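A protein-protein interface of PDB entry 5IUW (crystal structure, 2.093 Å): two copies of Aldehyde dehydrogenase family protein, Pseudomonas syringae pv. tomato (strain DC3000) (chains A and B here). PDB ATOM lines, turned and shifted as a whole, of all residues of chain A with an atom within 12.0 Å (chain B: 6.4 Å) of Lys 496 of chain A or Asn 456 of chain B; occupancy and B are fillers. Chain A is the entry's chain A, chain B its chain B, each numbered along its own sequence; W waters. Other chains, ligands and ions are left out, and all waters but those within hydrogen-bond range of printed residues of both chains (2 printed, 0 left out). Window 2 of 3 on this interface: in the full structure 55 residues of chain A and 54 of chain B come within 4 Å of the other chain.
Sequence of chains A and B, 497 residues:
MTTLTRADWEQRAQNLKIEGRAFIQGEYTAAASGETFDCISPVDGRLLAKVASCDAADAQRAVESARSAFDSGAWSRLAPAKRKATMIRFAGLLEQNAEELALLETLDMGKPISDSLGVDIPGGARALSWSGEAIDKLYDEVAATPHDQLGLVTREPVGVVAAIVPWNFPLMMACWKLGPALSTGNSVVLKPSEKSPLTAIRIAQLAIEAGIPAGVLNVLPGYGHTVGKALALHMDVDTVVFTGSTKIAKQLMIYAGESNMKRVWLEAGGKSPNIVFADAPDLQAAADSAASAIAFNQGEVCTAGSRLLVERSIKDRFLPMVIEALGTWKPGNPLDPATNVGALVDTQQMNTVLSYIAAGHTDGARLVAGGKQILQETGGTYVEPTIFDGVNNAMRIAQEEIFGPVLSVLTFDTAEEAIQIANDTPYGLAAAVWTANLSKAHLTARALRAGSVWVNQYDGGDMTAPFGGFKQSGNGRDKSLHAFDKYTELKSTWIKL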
ATOM      1  N   VAL A 142     -10.335 -41.386  13.077  1.00  0.00           N
ATOM      2  CA  VAL A 142     -10.411 -39.931  13.133  1.00  0.00           C
ATOM      3  C   VAL A 142      -9.971 -39.481  14.526  1.00  0.00           C
ATOM      4  O   VAL A 142     -10.562 -39.893  15.525  1.00  0.00           O
ATOM      5  CB  VAL A 142     -11.833 -39.402  12.867  1.00  0.00           C
ATOM      6  CG1 VAL A 142     -11.859 -37.870  12.970  1.00  0.00           C
ATOM      7  CG2 VAL A 142     -12.357 -39.893  11.520  1.00  0.00           C
ATOM      8  N   ALA A 143      -8.955 -38.632  14.591  1.00  0.00           N
ATOM      9  CA  ALA A 143      -8.385 -38.239  15.877  1.00  0.00           C
ATOM     10  C   ALA A 143      -9.230 -37.183  16.615  1.00  0.00           C
ATOM     11  O   ALA A 143      -9.957 -36.427  16.002  1.00  0.00           O
ATOM     12  CB  ALA A 143      -6.970 -37.731  15.669  1.00  0.00           C
ATOM     13  N   THR A 145      -9.291 -33.808  17.852  1.00  0.00           N
ATOM     14  CA  THR A 145      -8.527 -32.603  17.524  1.00  0.00           C
ATOM     15  C   THR A 145      -9.281 -31.330  17.917  1.00  0.00           C
ATOM     16  O   THR A 145     -10.480 -31.392  18.192  1.00  0.00           O
ATOM     17  CB  THR A 145      -8.238 -32.527  16.006  1.00  0.00           C
ATOM     18  OG1 THR A 145      -9.480 -32.497  15.280  1.00  0.00           O
ATOM     19  CG2 THR A 145      -7.383 -33.704  15.547  1.00  0.00           C
ATOM     20  N   PRO A 146      -8.592 -30.170  17.927  1.00  0.00           N
ATOM     21  CA  PRO A 146      -9.314 -28.899  18.090  1.00  0.00           C
ATOM     22  C   PRO A 146     -10.362 -28.678  16.998  1.00  0.00           C
ATOM     23  O   PRO A 146     -10.331 -29.348  15.968  1.00  0.00           O
ATOM     24  CB  PRO A 146      -8.205 -27.847  17.996  1.00  0.00           C
ATOM     25  CG  PRO A 146      -6.981 -28.556  18.436  1.00  0.00           C
ATOM     26  CD  PRO A 146      -7.132 -29.965  17.912  1.00  0.00           C
ATOM     27  N   HIS A 147     -11.264 -27.731  17.228  1.00  0.00           N
ATOM     28  CA  HIS A 147     -12.428 -27.522  16.378  1.00  0.00           C
ATOM     29  C   HIS A 147     -12.084 -27.111  14.942  1.00  0.00           C
ATOM     30  O   HIS A 147     -12.891 -27.304  14.036  1.00  0.00           O
ATOM     31  CB  HIS A 147     -13.331 -26.445  16.992  1.00  0.00           C
ATOM     32  CG  HIS A 147     -12.845 -25.047  16.744  1.00  0.00           C
ATOM     33  ND1 HIS A 147     -11.878 -24.444  17.526  1.00  0.00           N
ATOM     34  CD2 HIS A 147     -13.173 -24.140  15.794  1.00  0.00           C
ATOM     35  CE1 HIS A 147     -11.642 -23.227  17.072  1.00  0.00           C
ATOM     36  NE2 HIS A 147     -12.414 -23.016  16.023  1.00  0.00           N
ATOM     37  N   ASP A 148     -10.901 -26.535  14.735  1.00  0.00           N
ATOM     38  CA  ASP A 148     -10.519 -26.077  13.405  1.00  0.00           C
ATOM     39  C   ASP A 148      -9.591 -27.062  12.703  1.00  0.00           C
ATOM     40  O   ASP A 148      -8.886 -26.697  11.769  1.00  0.00           O
ATOM     41  CB  ASP A 148      -9.854 -24.700  13.481  1.00  0.00           C
ATOM     42  CG  ASP A 148      -8.567 -24.714  14.268  1.00  0.00           C
ATOM     43  OD1 ASP A 148      -8.356 -25.647  15.063  1.00  0.00           O
ATOM     44  OD2 ASP A 148      -7.764 -23.776  14.101  1.00  0.00           O
ATOM     45  N   GLN A 149      -9.577 -28.303  13.176  1.00  0.00           N
ATOM     46  CA  GLN A 149      -8.744 -29.343  12.579  1.00  0.00           C
ATOM     47  C   GLN A 149      -9.552 -30.596  12.337  1.00  0.00           C
ATOM     48  O   GLN A 149     -10.408 -30.942  13.138  1.00  0.00           O
ATOM     49  CB  GLN A 149      -7.550 -29.692  13.477  1.00  0.00           C
ATOM     50  CG  GLN A 149      -6.616 -28.542  13.782  1.00  0.00           C
ATOM     51  CD  GLN A 149      -5.573 -28.354  12.710  1.00  0.00           C
ATOM     52  OE1 GLN A 149      -5.196 -29.302  12.022  1.00  0.00           O
ATOM     53  NE2 GLN A 149      -5.111 -27.120  12.547  1.00  0.00           N
ATOM     54  N   LEU A 150      -9.275 -31.273  11.231  1.00  0.00           N
ATOM     55  CA  LEU A 150      -9.771 -32.624  11.031  1.00  0.00           C
ATOM     56  C   LEU A 150      -8.578 -33.543  10.831  1.00  0.00           C
ATOM     57  O   LEU A 150      -7.808 -33.372   9.887  1.00  0.00           O
ATOM     58  CB  LEU A 150     -10.724 -32.701   9.838  1.00  0.00           C
ATOM     59  CG  LEU A 150     -11.160 -34.108   9.405  1.00  0.00           C
ATOM     60  CD1 LEU A 150     -11.929 -34.772  10.516  1.00  0.00           C
ATOM     61  CD2 LEU A 150     -12.002 -34.088   8.109  1.00  0.00           C
ATOM     62  N   GLY A 151      -8.429 -34.516  11.722  1.00  0.00           N
ATOM     63  CA  GLY A 151      -7.282 -35.405  11.684  1.00  0.00           C
ATOM     64  C   GLY A 151      -7.652 -36.823  11.282  1.00  0.00           C
ATOM     65  O   GLY A 151      -8.247 -37.577  12.056  1.00  0.00           O
ATOM     66  N   LEU A 152      -7.302 -37.187  10.064  1.00  0.00           N
ATOM     67  CA  LEU A 152      -7.540 -38.543   9.586  1.00  0.00           C
ATOM     68  C   LEU A 152      -6.306 -39.444   9.683  1.00  0.00           C
ATOM     69  O   LEU A 152      -5.196 -39.051   9.323  1.00  0.00           O
ATOM     70  CB  LEU A 152      -8.026 -38.505   8.140  1.00  0.00           C
ATOM     71  CG  LEU A 152      -9.173 -37.540   7.850  1.00  0.00           C
ATOM     72  CD1 LEU A 152      -9.479 -37.512   6.374  1.00  0.00           C
ATOM     73  CD2 LEU A 152     -10.401 -37.952   8.686  1.00  0.00           C
ATOM     74  N   SER A 492      -1.245 -39.956   8.198  1.00  0.00           N
ATOM     75  CA  SER A 492      -1.934 -38.945   8.978  1.00  0.00           C
ATOM     76  C   SER A 492      -2.244 -37.735   8.096  1.00  0.00           C
ATOM     77  O   SER A 492      -1.334 -37.039   7.657  1.00  0.00           O
ATOM     78  CB  SER A 492      -1.087 -38.520  10.179  1.00  0.00           C
ATOM     79  OG  SER A 492      -0.941 -39.586  11.086  1.00  0.00           O
ATOM     80  N   THR A 493      -3.523 -37.503   7.811  1.00  0.00           N
ATOM     81  CA  THR A 493      -3.909 -36.318   7.069  1.00  0.00           C
ATOM     82  C   THR A 493      -4.521 -35.315   8.047  1.00  0.00           C
ATOM     83  O   THR A 493      -5.616 -35.530   8.563  1.00  0.00           O
ATOM     84  CB  THR A 493      -4.905 -36.644   5.918  1.00  0.00           C
ATOM     85  OG1 THR A 493      -4.372 -37.698   5.099  1.00  0.00           O
ATOM     86  CG2 THR A 493      -5.162 -35.411   5.062  1.00  0.00           C
ATOM     87  N   TRP A 494      -3.791 -34.239   8.316  1.00  0.00           N
ATOM     88  CA  TRP A 494      -4.252 -33.208   9.248  1.00  0.00           C
ATOM     89  C   TRP A 494      -4.676 -31.972   8.472  1.00  0.00           C
ATOM     90  O   TRP A 494      -3.861 -31.311   7.839  1.00  0.00           O
ATOM     91  CB  TRP A 494      -3.172 -32.866  10.295  1.00  0.00           C
ATOM     92  CG  TRP A 494      -3.547 -33.340  11.677  1.00  0.00           C
ATOM     93  CD1 TRP A 494      -3.834 -32.565  12.773  1.00  0.00           C
ATOM     94  CD2 TRP A 494      -3.740 -34.696  12.087  1.00  0.00           C
ATOM     95  NE1 TRP A 494      -4.172 -33.362  13.838  1.00  0.00           N
ATOM     96  CE2 TRP A 494      -4.119 -34.674  13.445  1.00  0.00           C
ATOM     97  CE3 TRP A 494      -3.620 -35.930  11.442  1.00  0.00           C
ATOM     98  CZ2 TRP A 494      -4.378 -35.835  14.164  1.00  0.00           C
ATOM     99  CZ3 TRP A 494      -3.875 -37.079  12.158  1.00  0.00           C
ATOM    100  CH2 TRP A 494      -4.257 -37.025  13.504  1.00  0.00           C
ATOM    101  N   ILE A 495      -5.971 -31.687   8.523  1.00  0.00           N
ATOM    102  CA  ILE A 495      -6.591 -30.670   7.704  1.00  0.00           C
ATOM    103  C   ILE A 495      -7.028 -29.455   8.516  1.00  0.00           C
ATOM    104  O   ILE A 495      -7.838 -29.579   9.433  1.00  0.00           O
ATOM    105  CB  ILE A 495      -7.839 -31.233   6.981  1.00  0.00           C
ATOM    106  CG1 ILE A 495      -7.476 -32.512   6.212  1.00  0.00           C
ATOM    107  CG2 ILE A 495      -8.446 -30.171   6.082  1.00  0.00           C
ATOM    108  CD1 ILE A 495      -8.664 -33.418   5.912  1.00  0.00           C
ATOM    109  N   LYS A 496      -6.518 -28.281   8.178  1.00  0.00           N
ATOM    110  CA  LYS A 496      -7.008 -27.088   8.847  1.00  0.00           C
ATOM    111  C   LYS A 496      -8.257 -26.563   8.158  1.00  0.00           C
ATOM    112  O   LYS A 496      -8.304 -26.430   6.926  1.00  0.00           O
ATOM    113  CB  LYS A 496      -5.943 -25.996   8.914  1.00  0.00           C
ATOM    114  CG  LYS A 496      -6.454 -24.738   9.591  1.00  0.00           C
ATOM    115  CD  LYS A 496      -5.343 -23.874  10.102  1.00  0.00           C
ATOM    116  CE  LYS A 496      -5.916 -22.666  10.817  1.00  0.00           C
ATOM    117  NZ  LYS A 496      -4.845 -21.914  11.501  1.00  0.00           N
ATOM    118  N   LEU A 497      -9.267 -26.283   8.972  1.00  0.00           N
ATOM    119  CA  LEU A 497     -10.554 -25.799   8.497  1.00  0.00           C
ATOM    120  C   LEU A 497     -10.710 -24.327   8.855  1.00  0.00           C
ATOM    121  O   LEU A 497     -11.529 -23.621   8.269  1.00  0.00           O
ATOM    122  CB  LEU A 497     -11.697 -26.621   9.106  1.00  0.00           C
ATOM    123  CG  LEU A 497     -11.588 -28.153   9.023  1.00  0.00           C
ATOM    124  CD1 LEU A 497     -12.633 -28.861   9.890  1.00  0.00           C
ATOM    125  CD2 LEU A 497     -11.697 -28.622   7.588  1.00  0.00           C
ATOM    126  N   ALA B 280      -5.463 -21.656  -3.079  1.00  0.00           N
ATOM    127  CA  ALA B 280      -5.214 -21.676  -1.636  1.00  0.00           C
ATOM    128  C   ALA B 280      -6.095 -20.626  -0.971  1.00  0.00           C
ATOM    129  O   ALA B 280      -6.278 -19.550  -1.516  1.00  0.00           O
ATOM    130  CB  ALA B 280      -3.734 -21.411  -1.324  1.00  0.00           C
ATOM    131  N   PRO B 281      -6.670 -20.948   0.192  1.00  0.00           N
ATOM    132  CA  PRO B 281      -7.592 -20.017   0.856  1.00  0.00           C
ATOM    133  C   PRO B 281      -6.916 -18.747   1.360  1.00  0.00           C
ATOM    134  O   PRO B 281      -7.540 -17.687   1.377  1.00  0.00           O
ATOM    135  CB  PRO B 281      -8.141 -20.833   2.029  1.00  0.00           C
ATOM    136  CG  PRO B 281      -7.190 -21.948   2.220  1.00  0.00           C
ATOM    137  CD  PRO B 281      -6.597 -22.248   0.877  1.00  0.00           C
ATOM    138  N   ALA B 285      -0.851 -16.733   4.484  1.00  0.00           N
ATOM    139  CA  ALA B 285      -0.622 -17.831   5.416  1.00  0.00           C
ATOM    140  C   ALA B 285       0.266 -18.889   4.767  1.00  0.00           C
ATOM    141  O   ALA B 285       1.168 -19.425   5.405  1.00  0.00           O
ATOM    142  CB  ALA B 285      -1.944 -18.440   5.876  1.00  0.00           C
ATOM    143  N   SER B 289       4.006 -19.849   6.186  1.00  0.00           N
ATOM    144  CA  SER B 289       4.250 -21.244   6.532  1.00  0.00           C
ATOM    145  C   SER B 289       5.355 -21.843   5.667  1.00  0.00           C
ATOM    146  O   SER B 289       6.121 -22.673   6.134  1.00  0.00           O
ATOM    147  CB  SER B 289       2.965 -22.069   6.405  1.00  0.00           C
ATOM    148  OG  SER B 289       1.995 -21.619   7.336  1.00  0.00           O
ATOM    149  N   ALA B 432       2.618 -31.384   2.067  1.00  0.00           N
ATOM    150  CA  ALA B 432       1.501 -30.484   2.345  1.00  0.00           C
ATOM    151  C   ALA B 432       0.780 -30.035   1.068  1.00  0.00           C
ATOM    152  O   ALA B 432       1.359 -30.003  -0.015  1.00  0.00           O
ATOM    153  CB  ALA B 432       1.973 -29.285   3.130  1.00  0.00           C
ATOM    154  N   VAL B 433      -0.496 -29.694   1.220  1.00  0.00           N
ATOM    155  CA  VAL B 433      -1.340 -29.288   0.112  1.00  0.00           C
ATOM    156  C   VAL B 433      -2.158 -28.073   0.507  1.00  0.00           C
ATOM    157  O   VAL B 433      -2.839 -28.095   1.529  1.00  0.00           O
ATOM    158  CB  VAL B 433      -2.306 -30.416  -0.322  1.00  0.00           C
ATOM    159  CG1 VAL B 433      -3.234 -29.916  -1.394  1.00  0.00           C
ATOM    160  CG2 VAL B 433      -1.540 -31.606  -0.824  1.00  0.00           C
ATOM    161  N   TRP B 434      -2.102 -27.024  -0.305  1.00  0.00           N
ATOM    162  CA  TRP B 434      -2.870 -25.821  -0.021  1.00  0.00           C
ATOM    163  C   TRP B 434      -3.908 -25.569  -1.115  1.00  0.00           C
ATOM    164  O   TRP B 434      -3.555 -25.214  -2.241  1.00  0.00           O
ATOM    165  CB  TRP B 434      -1.949 -24.610   0.128  1.00  0.00           C
ATOM    166  CG  TRP B 434      -0.902 -24.748   1.206  1.00  0.00           C
ATOM    167  CD1 TRP B 434       0.212 -25.535   1.172  1.00  0.00           C
ATOM    168  CD2 TRP B 434      -0.871 -24.062   2.470  1.00  0.00           C
ATOM    169  NE1 TRP B 434       0.935 -25.383   2.342  1.00  0.00           N
ATOM    170  CE2 TRP B 434       0.285 -24.488   3.152  1.00  0.00           C
ATOM    171  CE3 TRP B 434      -1.716 -23.133   3.090  1.00  0.00           C
ATOM    172  CZ2 TRP B 434       0.624 -24.009   4.421  1.00  0.00           C
ATOM    173  CZ3 TRP B 434      -1.384 -22.664   4.352  1.00  0.00           C
ATOM    174  CH2 TRP B 434      -0.223 -23.103   5.002  1.00  0.00           C
ATOM    175  N   THR B 435      -5.184 -25.753  -0.770  1.00  0.00           N
ATOM    176  CA  THR B 435      -6.296 -25.495  -1.682  1.00  0.00           C
ATOM    177  C   THR B 435      -7.617 -25.363  -0.921  1.00  0.00           C
ATOM    178  O   THR B 435      -7.823 -26.016   0.093  1.00  0.00           O
ATOM    179  CB  THR B 435      -6.445 -26.612  -2.767  1.00  0.00           C
ATOM    180  OG1 THR B 435      -7.689 -26.453  -3.458  1.00  0.00           O
ATOM    181  CG2 THR B 435      -6.439 -27.971  -2.148  1.00  0.00           C
ATOM    182  N   ALA B 436      -8.507 -24.517  -1.428  1.00  0.00           N
ATOM    183  CA  ALA B 436      -9.821 -24.327  -0.828  1.00  0.00           C
ATOM    184  C   ALA B 436     -10.864 -25.324  -1.344  1.00  0.00           C
ATOM    185  O   ALA B 436     -11.982 -25.358  -0.849  1.00  0.00           O
ATOM    186  CB  ALA B 436     -10.301 -22.902  -1.071  1.00  0.00           C
ATOM    187  N   ASN B 437     -10.501 -26.114  -2.348  1.00  0.00           N
ATOM    188  CA  ASN B 437     -11.457 -26.997  -3.016  1.00  0.00           C
ATOM    189  C   ASN B 437     -11.569 -28.341  -2.296  1.00  0.00           C
ATOM    190  O   ASN B 437     -10.568 -29.006  -2.056  1.00  0.00           O
ATOM    191  CB  ASN B 437     -11.050 -27.193  -4.486  1.00  0.00           C
ATOM    192  CG  ASN B 437     -12.066 -27.991  -5.279  1.00  0.00           C
ATOM    193  OD1 ASN B 437     -11.912 -29.191  -5.460  1.00  0.00           O
ATOM    194  ND2 ASN B 437     -13.107 -27.318  -5.765  1.00  0.00           N
ATOM    195  N   ALA B 441      -8.559 -31.165  -2.463  1.00  0.00           N
ATOM    196  CA  ALA B 441      -7.833 -31.347  -1.207  1.00  0.00           C
ATOM    197  C   ALA B 441      -7.712 -32.827  -0.849  1.00  0.00           C
ATOM    198  O   ALA B 441      -6.601 -33.340  -0.668  1.00  0.00           O
ATOM    199  CB  ALA B 441      -8.506 -30.588  -0.086  1.00  0.00           C
ATOM    200  N   TRP B 454      -0.274 -32.586   5.293  1.00  0.00           N
ATOM    201  CA  TRP B 454      -0.899 -31.445   5.941  1.00  0.00           C
ATOM    202  C   TRP B 454      -1.683 -30.637   4.909  1.00  0.00           C
ATOM    203  O   TRP B 454      -1.188 -30.362   3.816  1.00  0.00           O
ATOM    204  CB  TRP B 454       0.165 -30.601   6.653  1.00  0.00           C
ATOM    205  CG  TRP B 454       0.873 -31.395   7.714  1.00  0.00           C
ATOM    206  CD1 TRP B 454       0.288 -32.076   8.740  1.00  0.00           C
ATOM    207  CD2 TRP B 454       2.281 -31.616   7.840  1.00  0.00           C
ATOM    208  NE1 TRP B 454       1.239 -32.702   9.499  1.00  0.00           N
ATOM    209  CE2 TRP B 454       2.471 -32.440   8.969  1.00  0.00           C
ATOM    210  CE3 TRP B 454       3.399 -31.196   7.117  1.00  0.00           C
ATOM    211  CZ2 TRP B 454       3.733 -32.855   9.388  1.00  0.00           C
ATOM    212  CZ3 TRP B 454       4.662 -31.605   7.543  1.00  0.00           C
ATOM    213  CH2 TRP B 454       4.816 -32.417   8.667  1.00  0.00           C
ATOM    214  N   VAL B 455      -2.916 -30.281   5.247  1.00  0.00           N
ATOM    215  CA  VAL B 455      -3.759 -29.540   4.319  1.00  0.00           C
ATOM    216  C   VAL B 455      -4.064 -28.154   4.867  1.00  0.00           C
ATOM    217  O   VAL B 455      -4.589 -28.016   5.973  1.00  0.00           O
ATOM    218  CB  VAL B 455      -5.085 -30.275   4.014  1.00  0.00           C
ATOM    219  CG1 VAL B 455      -5.944 -29.455   3.031  1.00  0.00           C
ATOM    220  CG2 VAL B 455      -4.813 -31.679   3.462  1.00  0.00           C
ATOM    221  N   ASN B 456      -3.708 -27.140   4.084  1.00  0.00           N
ATOM    222  CA  ASN B 456      -3.884 -25.733   4.452  1.00  0.00           C
ATOM    223  C   ASN B 456      -3.174 -25.359   5.754  1.00  0.00           C
ATOM    224  O   ASN B 456      -3.603 -24.482   6.496  1.00  0.00           O
ATOM    225  CB  ASN B 456      -5.378 -25.400   4.508  1.00  0.00           C
ATOM    226  CG  ASN B 456      -6.015 -25.465   3.132  1.00  0.00           C
ATOM    227  OD1 ASN B 456      -5.324 -25.316   2.125  1.00  0.00           O
ATOM    228  ND2 ASN B 456      -7.318 -25.717   3.076  1.00  0.00           N
ATOM    229  N   GLN B 457      -2.068 -26.039   6.002  1.00  0.00           N
ATOM    230  CA  GLN B 457      -1.188 -25.733   7.111  1.00  0.00           C
ATOM    231  C   GLN B 457       0.112 -26.479   6.847  1.00  0.00           C
ATOM    232  O   GLN B 457       0.178 -27.287   5.930  1.00  0.00           O
ATOM    233  CB  GLN B 457      -1.809 -26.146   8.448  1.00  0.00           C
ATOM    234  CG  GLN B 457      -1.928 -27.650   8.631  1.00  0.00           C
ATOM    235  CD  GLN B 457      -2.781 -28.018   9.824  1.00  0.00           C
ATOM    236  OE1 GLN B 457      -2.679 -27.408  10.882  1.00  0.00           O
ATOM    237  NE2 GLN B 457      -3.647 -29.007   9.652  1.00  0.00           N
ATOM    238  N   TYR B 458       1.149 -26.193   7.623  1.00  0.00           N
ATOM    239  CA  TYR B 458       2.353 -27.019   7.570  1.00  0.00           C
ATOM    240  C   TYR B 458       2.742 -27.409   8.981  1.00  0.00           C
ATOM    241  O   TYR B 458       2.462 -26.683   9.925  1.00  0.00           O
ATOM    242  CB  TYR B 458       3.521 -26.309   6.880  1.00  0.00           C
ATOM    243  CG  TYR B 458       4.546 -27.298   6.359  1.00  0.00           C
ATOM    244  CD1 TYR B 458       4.378 -27.896   5.127  1.00  0.00           C
ATOM    245  CD2 TYR B 458       5.652 -27.666   7.120  1.00  0.00           C
ATOM    246  CE1 TYR B 458       5.266 -28.817   4.652  1.00  0.00           C
ATOM    247  CE2 TYR B 458       6.563 -28.603   6.647  1.00  0.00           C
ATOM    248  CZ  TYR B 458       6.353 -29.176   5.402  1.00  0.00           C
ATOM    249  OH  TYR B 458       7.217 -30.108   4.881  1.00  0.00           O
HETATM  250  O   HOH W   1      -9.180 -24.756   5.050  1.00  0.00           O
HETATM  251  O   HOH W   2      -2.304 -29.292  13.357  1.00  0.00           O
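The backbone carbonyl oxygen of Gln 149 of chain A lies within hydrogen-bond range of the side-chain hydroxyl of Thr 145 of chain A, 2.8 Å away.
O of Leu 150 of chain A sits at hydrogen-bond distance from N of Ile 495 of chain A (2.8 Å).
The backbone carbonyl oxygen of Trp 454 of chain B is in hydrogen-bond range of the backbone NH of Val 433 of chain B.
N of Asn 456 of chain B sits at hydrogen-bond distance from O of Val 433 of chain B, at 2.9 Å.
The backbone NH (N) of Thr 435 of chain B sits at hydrogen-bond distance from the side-chain amide oxygen (OD1) of Asn 456 of chain B (2.9 Å).
Of the 16 printed residues of chain A, 4 touch a printed residue of chain B.
Hydrophobic or aromatic side chains of chain A within 4 Å of the printed part of chain B: Trp 494 and Ile 495.
Along chain A the printed residues that touch a printed residue of chain B span positions 149 to 496.
Hydrophobic or aromatic side chains of chain B within 4 Å of the printed part of chain A: Trp 454 and Val 455.
Among the printed residues, no Asp or Glu carboxylate lies within 4 Å of a Lys or Arg side-chain nitrogen of the other chain.
No position is printed for both chains.
Of chain B, only Val 455, Asn 456 and Gln 457 come within 4 Å of Lys 496 of chain A.
Asn 456 of chain B touches just one residue of chain A: Lys 496.
No residue of chain A comes within 4 Å of Ala 280 of chain B.
No residue of chain A comes within 4 Å of Trp 434 of chain B.
No residue of chain A comes within 4 Å of Thr 435 of chain B.
Ala 436 of chain B touches none of the printed residues of chain A.
Val 455 of chain B touches just these residues of chain A: Trp 494, Ile 495 and Lys 496.
Gln 457 of chain B touches just these residues of chain A: Gln 149 (2.8 Å), Trp 494 (2.9 Å), Ile 495 (3.6 Å) and Lys 496 (3.3 Å).
Of the printed residues of chain B, Ile 495 of chain A touches Val 455 and Gln 457.
Of the printed residues of chain B, Gln 149 of chain A touches Gln 457 (2.8 Å).
The nearest residue of chain B that does not touch Lys 496 of chain A is Trp 454 of chain B (6.3 Å).
The nearest residue of chain A that does not touch Asn 456 of chain B is Ile 495 of chain A (5.5 Å).
Water W1 lies within hydrogen-bond range of O of Lys 496 of chain A and ND2 of Asn 456 of chain B.
Water W2 lies within hydrogen-bond range of OE1 of Gln 457 of chain B (3.1 Å) and OE1 of Gln 149 of chain A (3.2 Å).
Among the printed residues, merely in contact across the chains: Trp 494 of chain A with Trp 454 of chain B (3.5 Å), Ile 495 of chain A with Val 455 of chain B (3.7 Å), Ile 495 of chain A with Gln 457 of chain B (3.6 Å) and Lys 496 of chain A with Asn 456 of chain B (3.7 Å).
OE1 of Gln 149 of chain A sits at hydrogen-bond distance from NE2 of Gln 457 of chain B (2.8 Å).
O of Trp 494 of chain A is in hydrogen-bond range of N of Val 455 of chain B (2.9 Å).
NE2 of Gln 457 of chain B sits at hydrogen-bond distance from O of Trp 494 of chain A (2.9 Å).
O of Val 455 of chain B lies within hydrogen-bond range of N of Lys 496 of chain A (2.9 Å).
NE2 of Gln 457 of chain B lies close to N of Lys 496 of chain A, 3.3 Å away.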
